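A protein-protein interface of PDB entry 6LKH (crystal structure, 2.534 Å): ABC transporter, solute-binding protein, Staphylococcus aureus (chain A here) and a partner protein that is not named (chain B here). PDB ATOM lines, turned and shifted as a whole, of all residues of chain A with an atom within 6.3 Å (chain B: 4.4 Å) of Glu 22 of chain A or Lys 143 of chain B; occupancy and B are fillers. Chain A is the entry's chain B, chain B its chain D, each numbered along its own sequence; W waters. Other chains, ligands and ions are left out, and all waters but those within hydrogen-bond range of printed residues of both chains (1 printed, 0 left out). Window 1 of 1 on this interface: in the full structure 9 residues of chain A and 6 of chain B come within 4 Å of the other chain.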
ATOM      1  N   ARG A  15     -20.263  18.055  31.609  1.00  0.00           N
ATOM      2  CA  ARG A  15     -21.378  18.033  30.667  1.00  0.00           C
ATOM      3  C   ARG A  15     -22.545  17.196  31.172  1.00  0.00           C
ATOM      4  O   ARG A  15     -23.693  17.656  31.047  1.00  0.00           O
ATOM      5  CB  ARG A  15     -20.897  17.533  29.302  1.00  0.00           C
ATOM      6  CG  ARG A  15     -21.844  17.829  28.147  1.00  0.00           C
ATOM      7  CD  ARG A  15     -22.053  19.314  27.942  1.00  0.00           C
ATOM      8  NE  ARG A  15     -23.265  19.795  28.596  1.00  0.00           N
ATOM      9  CZ  ARG A  15     -23.770  21.015  28.436  1.00  0.00           C
ATOM     10  NH1 ARG A  15     -23.171  21.891  27.638  1.00  0.00           N
ATOM     11  NH2 ARG A  15     -24.878  21.360  29.074  1.00  0.00           N
ATOM     12  N   ILE A  17     -23.585  16.513  34.316  1.00  0.00           N
ATOM     13  CA  ILE A  17     -24.312  17.054  35.462  1.00  0.00           C
ATOM     14  C   ILE A  17     -24.954  18.387  35.100  1.00  0.00           C
ATOM     15  O   ILE A  17     -26.047  18.703  35.587  1.00  0.00           O
ATOM     16  CB  ILE A  17     -23.410  17.168  36.713  1.00  0.00           C
ATOM     17  CG1 ILE A  17     -22.560  18.444  36.705  1.00  0.00           C
ATOM     18  CG2 ILE A  17     -22.514  15.931  36.845  1.00  0.00           C
ATOM     19  CD1 ILE A  17     -21.893  18.730  38.036  1.00  0.00           C
ATOM     20  N   LEU A  18     -24.310  19.180  34.238  1.00  0.00           N
ATOM     21  CA  LEU A  18     -24.954  20.398  33.757  1.00  0.00           C
ATOM     22  C   LEU A  18     -26.170  20.062  32.901  1.00  0.00           C
ATOM     23  O   LEU A  18     -27.185  20.768  32.954  1.00  0.00           O
ATOM     24  CB  LEU A  18     -23.954  21.257  32.982  1.00  0.00           C
ATOM     25  CG  LEU A  18     -22.820  21.877  33.804  1.00  0.00           C
ATOM     26  CD1 LEU A  18     -21.848  22.603  32.898  1.00  0.00           C
ATOM     27  CD2 LEU A  18     -23.353  22.826  34.867  1.00  0.00           C
ATOM     28  N   ASN A  19     -26.091  18.980  32.115  1.00  0.00           N
ATOM     29  CA  ASN A  19     -27.267  18.507  31.387  1.00  0.00           C
ATOM     30  C   ASN A  19     -28.429  18.252  32.334  1.00  0.00           C
ATOM     31  O   ASN A  19     -29.567  18.645  32.054  1.00  0.00           O
ATOM     32  CB  ASN A  19     -26.943  17.231  30.609  1.00  0.00           C
ATOM     33  CG  ASN A  19     -26.077  17.493  29.396  1.00  0.00           C
ATOM     34  OD1 ASN A  19     -25.947  18.635  28.947  1.00  0.00           O
ATOM     35  ND2 ASN A  19     -25.482  16.438  28.853  1.00  0.00           N
ATOM     36  N   GLU A  20     -28.159  17.597  33.466  1.00  0.00           N
ATOM     37  CA  GLU A  20     -29.215  17.338  34.438  1.00  0.00           C
ATOM     38  C   GLU A  20     -29.786  18.631  34.998  1.00  0.00           C
ATOM     39  O   GLU A  20     -30.963  18.678  35.369  1.00  0.00           O
ATOM     40  CB  GLU A  20     -28.688  16.454  35.568  1.00  0.00           C
ATOM     41  CG  GLU A  20     -29.664  16.265  36.727  1.00  0.00           C
ATOM     42  CD  GLU A  20     -31.036  15.795  36.275  1.00  0.00           C
ATOM     43  OE1 GLU A  20     -31.125  15.146  35.213  1.00  0.00           O
ATOM     44  OE2 GLU A  20     -32.025  16.078  36.985  1.00  0.00           O
ATOM     45  N   PHE A  21     -28.972  19.686  35.071  1.00  0.00           N
ATOM     46  CA  PHE A  21     -29.479  20.987  35.488  1.00  0.00           C
ATOM     47  C   PHE A  21     -30.290  21.657  34.390  1.00  0.00           C
ATOM     48  O   PHE A  21     -31.258  22.365  34.686  1.00  0.00           O
ATOM     49  CB  PHE A  21     -28.321  21.896  35.898  1.00  0.00           C
ATOM     50  CG  PHE A  21     -28.752  23.255  36.376  1.00  0.00           C
ATOM     51  CD1 PHE A  21     -29.072  23.463  37.704  1.00  0.00           C
ATOM     52  CD2 PHE A  21     -28.825  24.325  35.499  1.00  0.00           C
ATOM     53  CE1 PHE A  21     -29.459  24.712  38.152  1.00  0.00           C
ATOM     54  CE2 PHE A  21     -29.213  25.576  35.940  1.00  0.00           C
ATOM     55  CZ  PHE A  21     -29.528  25.770  37.268  1.00  0.00           C
ATOM     56  N   GLU A  22     -29.906  21.458  33.128  1.00  0.00           N
ATOM     57  CA  GLU A  22     -30.647  22.064  32.028  1.00  0.00           C
ATOM     58  C   GLU A  22     -32.117  21.664  32.071  1.00  0.00           C
ATOM     59  O   GLU A  22     -33.004  22.523  32.035  1.00  0.00           O
ATOM     60  CB  GLU A  22     -30.021  21.664  30.692  1.00  0.00           C
ATOM     61  CG  GLU A  22     -28.735  22.399  30.348  1.00  0.00           C
ATOM     62  CD  GLU A  22     -28.224  22.045  28.967  1.00  0.00           C
ATOM     63  OE1 GLU A  22     -28.470  20.904  28.521  1.00  0.00           O
ATOM     64  OE2 GLU A  22     -27.587  22.905  28.327  1.00  0.00           O
ATOM     65  N   LYS A  23     -32.395  20.361  32.153  1.00  0.00           N
ATOM     66  CA  LYS A  23     -33.764  19.867  32.123  1.00  0.00           C
ATOM     67  C   LYS A  23     -34.365  19.709  33.514  1.00  0.00           C
ATOM     68  O   LYS A  23     -35.452  19.140  33.651  1.00  0.00           O
ATOM     69  CB  LYS A  23     -33.847  18.547  31.340  1.00  0.00           C
ATOM     70  CG  LYS A  23     -32.871  17.446  31.717  1.00  0.00           C
ATOM     71  CD  LYS A  23     -32.829  16.394  30.605  1.00  0.00           C
ATOM     72  CE  LYS A  23     -31.506  15.650  30.558  1.00  0.00           C
ATOM     73  NZ  LYS A  23     -31.507  14.585  29.516  1.00  0.00           N
ATOM     74  N   GLN A  24     -33.691  20.210  34.544  1.00  0.00           N
ATOM     75  CA  GLN A  24     -34.322  20.420  35.838  1.00  0.00           C
ATOM     76  C   GLN A  24     -34.838  21.842  35.983  1.00  0.00           C
ATOM     77  O   GLN A  24     -35.876  22.055  36.618  1.00  0.00           O
ATOM     78  CB  GLN A  24     -33.335  20.107  36.968  1.00  0.00           C
ATOM     79  CG  GLN A  24     -33.699  20.715  38.312  1.00  0.00           C
ATOM     80  CD  GLN A  24     -32.809  20.218  39.435  1.00  0.00           C
ATOM     81  OE1 GLN A  24     -32.481  19.033  39.509  1.00  0.00           O
ATOM     82  NE2 GLN A  24     -32.412  21.126  40.316  1.00  0.00           N
ATOM     83  N   GLU A  25     -34.142  22.814  35.390  1.00  0.00           N
ATOM     84  CA  GLU A  25     -34.513  24.220  35.484  1.00  0.00           C
ATOM     85  C   GLU A  25     -34.916  24.830  34.148  1.00  0.00           C
ATOM     86  O   GLU A  25     -35.222  26.027  34.098  1.00  0.00           O
ATOM     87  CB  GLU A  25     -33.353  25.032  36.077  1.00  0.00           C
ATOM     88  CG  GLU A  25     -32.835  24.504  37.403  1.00  0.00           C
ATOM     89  CD  GLU A  25     -33.862  24.585  38.512  1.00  0.00           C
ATOM     90  OE1 GLU A  25     -34.817  25.382  38.385  1.00  0.00           O
ATOM     91  OE2 GLU A  25     -33.715  23.852  39.513  1.00  0.00           O
ATOM     92  N   HIS A  26     -34.924  24.050  33.067  1.00  0.00           N
ATOM     93  CA  HIS A  26     -35.312  24.536  31.743  1.00  0.00           C
ATOM     94  C   HIS A  26     -34.421  25.701  31.308  1.00  0.00           C
ATOM     95  O   HIS A  26     -34.877  26.814  31.034  1.00  0.00           O
ATOM     96  CB  HIS A  26     -36.792  24.922  31.730  1.00  0.00           C
ATOM     97  CG  HIS A  26     -37.684  23.873  32.315  1.00  0.00           C
ATOM     98  ND1 HIS A  26     -38.007  22.712  31.647  1.00  0.00           N
ATOM     99  CD2 HIS A  26     -38.303  23.800  33.518  1.00  0.00           C
ATOM    100  CE1 HIS A  26     -38.797  21.974  32.407  1.00  0.00           C
ATOM    101  NE2 HIS A  26     -38.993  22.613  33.548  1.00  0.00           N
ATOM    102  N   VAL A  27     -33.124  25.411  31.249  1.00  0.00           N
ATOM    103  CA  VAL A  27     -32.103  26.373  30.866  1.00  0.00           C
ATOM    104  C   VAL A  27     -31.219  25.721  29.819  1.00  0.00           C
ATOM    105  O   VAL A  27     -31.050  24.498  29.797  1.00  0.00           O
ATOM    106  CB  VAL A  27     -31.250  26.829  32.072  1.00  0.00           C
ATOM    107  CG1 VAL A  27     -30.336  27.976  31.677  1.00  0.00           C
ATOM    108  CG2 VAL A  27     -32.136  27.226  33.238  1.00  0.00           C
ATOM    109  N   LYS A  28     -30.660  26.544  28.941  1.00  0.00           N
ATOM    110  CA  LYS A  28     -29.578  26.125  28.064  1.00  0.00           C
ATOM    111  C   LYS A  28     -28.263  26.590  28.669  1.00  0.00           C
ATOM    112  O   LYS A  28     -28.113  27.771  29.002  1.00  0.00           O
ATOM    113  CB  LYS A  28     -29.747  26.694  26.655  1.00  0.00           C
ATOM    114  CG  LYS A  28     -30.857  26.034  25.856  1.00  0.00           C
ATOM    115  CD  LYS A  28     -30.374  25.508  24.509  1.00  0.00           C
ATOM    116  CE  LYS A  28     -31.314  25.913  23.382  1.00  0.00           C
ATOM    117  NZ  LYS A  28     -30.951  25.279  22.082  1.00  0.00           N
ATOM    118  N   ILE A  29     -27.325  25.663  28.826  1.00  0.00           N
ATOM    119  CA  ILE A  29     -26.002  25.972  29.353  1.00  0.00           C
ATOM    120  C   ILE A  29     -24.978  25.725  28.253  1.00  0.00           C
ATOM    121  O   ILE A  29     -24.883  24.616  27.714  1.00  0.00           O
ATOM    122  CB  ILE A  29     -25.683  25.153  30.615  1.00  0.00           C
ATOM    123  CG1 ILE A  29     -26.447  25.727  31.816  1.00  0.00           C
ATOM    124  CG2 ILE A  29     -24.178  25.155  30.902  1.00  0.00           C
ATOM    125  CD1 ILE A  29     -26.349  24.897  33.082  1.00  0.00           C
ATOM    126  N   GLU A  30     -24.211  26.762  27.930  1.00  0.00           N
ATOM    127  CA  GLU A  30     -23.059  26.650  27.050  1.00  0.00           C
ATOM    128  C   GLU A  30     -21.785  26.678  27.881  1.00  0.00           C
ATOM    129  O   GLU A  30     -21.675  27.448  28.839  1.00  0.00           O
ATOM    130  CB  GLU A  30     -23.025  27.788  26.028  1.00  0.00           C
ATOM    131  CG  GLU A  30     -24.073  27.670  24.946  1.00  0.00           C
ATOM    132  CD  GLU A  30     -24.030  28.821  23.960  1.00  0.00           C
ATOM    133  OE1 GLU A  30     -23.156  29.701  24.107  1.00  0.00           O
ATOM    134  OE2 GLU A  30     -24.875  28.846  23.039  1.00  0.00           O
ATOM    135  N   TYR B 127     -32.715  21.106  24.369  1.00  0.00           N
ATOM    136  CA  TYR B 127     -31.443  21.573  24.898  1.00  0.00           C
ATOM    137  C   TYR B 127     -30.281  21.235  23.975  1.00  0.00           C
ATOM    138  O   TYR B 127     -29.123  21.301  24.398  1.00  0.00           O
ATOM    139  CB  TYR B 127     -31.213  20.981  26.288  1.00  0.00           C
ATOM    140  CG  TYR B 127     -32.364  21.227  27.231  1.00  0.00           C
ATOM    141  CD1 TYR B 127     -32.596  22.489  27.757  1.00  0.00           C
ATOM    142  CD2 TYR B 127     -33.218  20.198  27.592  1.00  0.00           C
ATOM    143  CE1 TYR B 127     -33.650  22.719  28.617  1.00  0.00           C
ATOM    144  CE2 TYR B 127     -34.275  20.416  28.447  1.00  0.00           C
ATOM    145  CZ  TYR B 127     -34.487  21.677  28.959  1.00  0.00           C
ATOM    146  OH  TYR B 127     -35.544  21.884  29.812  1.00  0.00           O
ATOM    147  N   ASP B 128     -30.570  20.866  22.727  1.00  0.00           N
ATOM    148  CA  ASP B 128     -29.594  20.587  21.676  1.00  0.00           C
ATOM    149  C   ASP B 128     -28.846  19.274  21.879  1.00  0.00           C
ATOM    150  O   ASP B 128     -27.888  19.000  21.142  1.00  0.00           O
ATOM    151  CB  ASP B 128     -28.581  21.729  21.518  1.00  0.00           C
ATOM    152  CG  ASP B 128     -29.221  23.029  21.057  1.00  0.00           C
ATOM    153  OD1 ASP B 128     -30.300  22.985  20.429  1.00  0.00           O
ATOM    154  OD2 ASP B 128     -28.639  24.101  21.317  1.00  0.00           O
ATOM    155  N   ASN B 129     -29.247  18.450  22.849  1.00  0.00           N
ATOM    156  CA  ASN B 129     -28.683  17.107  22.965  1.00  0.00           C
ATOM    157  C   ASN B 129     -29.052  16.276  21.741  1.00  0.00           C
ATOM    158  O   ASN B 129     -30.208  16.263  21.309  1.00  0.00           O
ATOM    159  CB  ASN B 129     -29.189  16.416  24.231  1.00  0.00           C
ATOM    160  CG  ASN B 129     -28.725  17.101  25.497  1.00  0.00           C
ATOM    161  OD1 ASN B 129     -27.527  17.309  25.705  1.00  0.00           O
ATOM    162  ND2 ASN B 129     -29.676  17.462  26.352  1.00  0.00           N
ATOM    163  N   ILE B 130     -28.069  15.577  21.187  1.00  0.00           N
ATOM    164  CA  ILE B 130     -28.293  14.752  20.006  1.00  0.00           C
ATOM    165  C   ILE B 130     -28.892  13.420  20.436  1.00  0.00           C
ATOM    166  O   ILE B 130     -28.287  12.681  21.219  1.00  0.00           O
ATOM    167  CB  ILE B 130     -26.990  14.549  19.222  1.00  0.00           C
ATOM    168  CG1 ILE B 130     -26.500  15.895  18.691  1.00  0.00           C
ATOM    169  CG2 ILE B 130     -27.196  13.552  18.071  1.00  0.00           C
ATOM    170  CD1 ILE B 130     -25.131  15.845  18.115  1.00  0.00           C
ATOM    171  N   GLU B 142     -24.160  13.841  22.783  1.00  0.00           N
ATOM    172  CA  GLU B 142     -23.428  15.094  22.721  1.00  0.00           C
ATOM    173  C   GLU B 142     -24.354  16.216  22.254  1.00  0.00           C
ATOM    174  O   GLU B 142     -25.537  16.008  21.974  1.00  0.00           O
ATOM    175  CB  GLU B 142     -22.220  14.955  21.799  1.00  0.00           C
ATOM    176  CG  GLU B 142     -21.294  13.812  22.171  1.00  0.00           C
ATOM    177  CD  GLU B 142     -20.007  13.810  21.369  1.00  0.00           C
ATOM    178  OE1 GLU B 142     -19.992  14.390  20.262  1.00  0.00           O
ATOM    179  OE2 GLU B 142     -19.011  13.226  21.845  1.00  0.00           O
ATOM    180  N   LYS B 143     -23.808  17.426  22.164  1.00  0.00           N
ATOM    181  CA  LYS B 143     -24.585  18.611  21.829  1.00  0.00           C
ATOM    182  C   LYS B 143     -24.459  18.937  20.348  1.00  0.00           C
ATOM    183  O   LYS B 143     -23.386  18.785  19.755  1.00  0.00           O
ATOM    184  CB  LYS B 143     -24.125  19.816  22.653  1.00  0.00           C
ATOM    185  CG  LYS B 143     -24.380  19.693  24.150  1.00  0.00           C
ATOM    186  CD  LYS B 143     -25.827  19.959  24.520  1.00  0.00           C
ATOM    187  CE  LYS B 143     -25.956  20.188  26.015  1.00  0.00           C
ATOM    188  NZ  LYS B 143     -27.344  19.997  26.508  1.00  0.00           N
ATOM    189  N   TYR B 144     -25.566  19.384  19.756  1.00  0.00           N
ATOM    190  CA  TYR B 144     -25.571  19.917  18.398  1.00  0.00           C
ATOM    191  C   TYR B 144     -25.539  21.436  18.482  1.00  0.00           C
ATOM    192  O   TYR B 144     -26.505  22.062  18.930  1.00  0.00           O
ATOM    193  CB  TYR B 144     -26.798  19.456  17.615  1.00  0.00           C
ATOM    194  CG  TYR B 144     -26.876  20.064  16.229  1.00  0.00           C
ATOM    195  CD1 TYR B 144     -25.936  19.740  15.257  1.00  0.00           C
ATOM    196  CD2 TYR B 144     -27.881  20.964  15.892  1.00  0.00           C
ATOM    197  CE1 TYR B 144     -25.996  20.294  13.988  1.00  0.00           C
ATOM    198  CE2 TYR B 144     -27.950  21.520  14.624  1.00  0.00           C
ATOM    199  CZ  TYR B 144     -27.003  21.181  13.676  1.00  0.00           C
ATOM    200  OH  TYR B 144     -27.060  21.731  12.414  1.00  0.00           O
ATOM    201  N   ARG B 145     -24.430  22.025  18.045  1.00  0.00           N
ATOM    202  CA  ARG B 145     -24.307  23.476  17.977  1.00  0.00           C
ATOM    203  C   ARG B 145     -24.429  23.909  16.523  1.00  0.00           C
ATOM    204  O   ARG B 145     -23.476  23.743  15.745  1.00  0.00           O
ATOM    205  CB  ARG B 145     -22.975  23.934  18.576  1.00  0.00           C
ATOM    206  CG  ARG B 145     -22.844  23.646  20.072  1.00  0.00           C
ATOM    207  CD  ARG B 145     -24.061  24.143  20.852  1.00  0.00           C
ATOM    208  NE  ARG B 145     -23.911  23.999  22.298  1.00  0.00           N
ATOM    209  CZ  ARG B 145     -24.920  24.060  23.163  1.00  0.00           C
ATOM    210  NH1 ARG B 145     -26.162  24.254  22.737  1.00  0.00           N
ATOM    211  NH2 ARG B 145     -24.690  23.920  24.461  1.00  0.00           N
HETATM  212  O   HOH W   1     -29.782  18.486  28.842  1.00  0.00           O
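Among the printed residues, pairs that only touch across the chains: Arg 15 of chain A with Lys 143 of chain B (3.4 Å), Asn 19 of chain A with Asn 129 of chain B (3.8 Å), Lys 23 of chain A with Tyr 127 of chain B (3.5 Å), Val 27 of chain A with Tyr 127 of chain B (3.3 Å) and Glu 30 of chain A with Arg 145 of chain B (3.8 Å).
Water W1 lies within hydrogen-bond range of ND2 of Asn 129 of chain B (2.7 Å), OE1 of Glu 22 of chain A (2.8 Å) and O of Asn 19 of chain A (3.2 Å).
OD1 of Asn 19 of chain A lies within hydrogen-bond range of NZ of Lys 143 of chain B, at 3.1 Å.
The backbone carbonyl oxygen (O) of Ile 29 of chain A is in hydrogen-bond range of the guanidinium group (NH2) of Arg 145 of chain B (3.3 Å).
The side-chain amino group of Lys 143 of chain B lies within salt-bridge range of the side-chain carboxylate of Glu 22 of chain A (2.5 Å).
The backbone carbonyl oxygen (O) of Glu 22 of chain A lies within hydrogen-bond range of the side-chain hydroxyl (OH) of Tyr 127 of chain B.
The side-chain amino group (NZ) of Lys 28 of chain A is in salt-bridge range of the side-chain carboxylate (OD2) of Asp 128 of chain B.
OH of Tyr 127 of chain B lies within hydrogen-bond range of ND1 of His 26 of chain A, at 3.2 Å.
Of chain B, only Tyr 127 and Lys 143 come within 4 Å of Glu 22 of chain A.
Gln 24 of chain A touches none of the printed residues of chain B.
Glu 25 of chain A touches none of the printed residues of chain B.
Of the printed residues of chain B, Ile 29 of chain A touches Arg 145 (3.3 Å).
Lys 143 of chain B touches just these residues of chain A: Arg 15 (3.4 Å), Asn 19 (3.1 Å) and Glu 22 (2.5 Å).
Printed residues of chain A within 4 Å of Arg 145 of chain B: Ile 29 (3.3 Å) and Glu 30 (3.8 Å).
The nearest printed residue of chain B that does not touch Ile 29 of chain A is Lys 143 of chain B (4.9 Å).
N of Ile 29 of chain A is in hydrogen-bond range of OE2 of Glu 22 of chain A, at 2.8 Å.
NH1 of Arg 15 of chain A lies within hydrogen-bond range of O of Ile 29 of chain A, 3.2 Å away.
O of Asp 128 of chain B sits at hydrogen-bond distance from N of Tyr 144 of chain B (2.7 Å).
The guanidinium group (NH2) of Arg 15 of chain A lies within hydrogen-bond range of the side-chain amide oxygen (OD1) of Asn 19 of chain A, 2.9 Å away.
NZ of Lys 143 of chain B sits at hydrogen-bond distance from OD1 of Asn 129 of chain B (2.8 Å).
The side-chain amide oxygen (OD1) of Asn 19 of chain A lies close to the side-chain carboxylate (OE1) of Glu 22 of chain A (3.4 Å).
Of the 15 printed residues of chain A, 9 touch a printed residue of chain B.
Printed residues of chain A that touch a printed residue of chain B: Arg 15, Asn 19, Glu 22, Lys 23, His 26, Val 27, Lys 28, Ile 29 and Glu 30.
Along chain A the printed residues that touch a printed residue of chain B span positions 15 to 30.
Of the 8 printed residues of chain B, 5 touch a printed residue of chain A.
Printed residues of chain B that touch a printed residue of chain A: Tyr 127, Asp 128, Asn 129, Lys 143 and Arg 145.
Hydrophobic or aromatic side chains of chain B within 4 Å of the printed part of chain A: Tyr 127.
Among the printed residues, 11 pairs touch across the chains.
Among the printed residues, Asp or Glu carboxylates within 4 Å of a Lys or Arg side-chain nitrogen of the other chain: Glu 22 of chain A with Lys 143 of chain B (2.5 Å) and Lys 28 of chain A with Asp 128 of chain B (2.7 Å).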
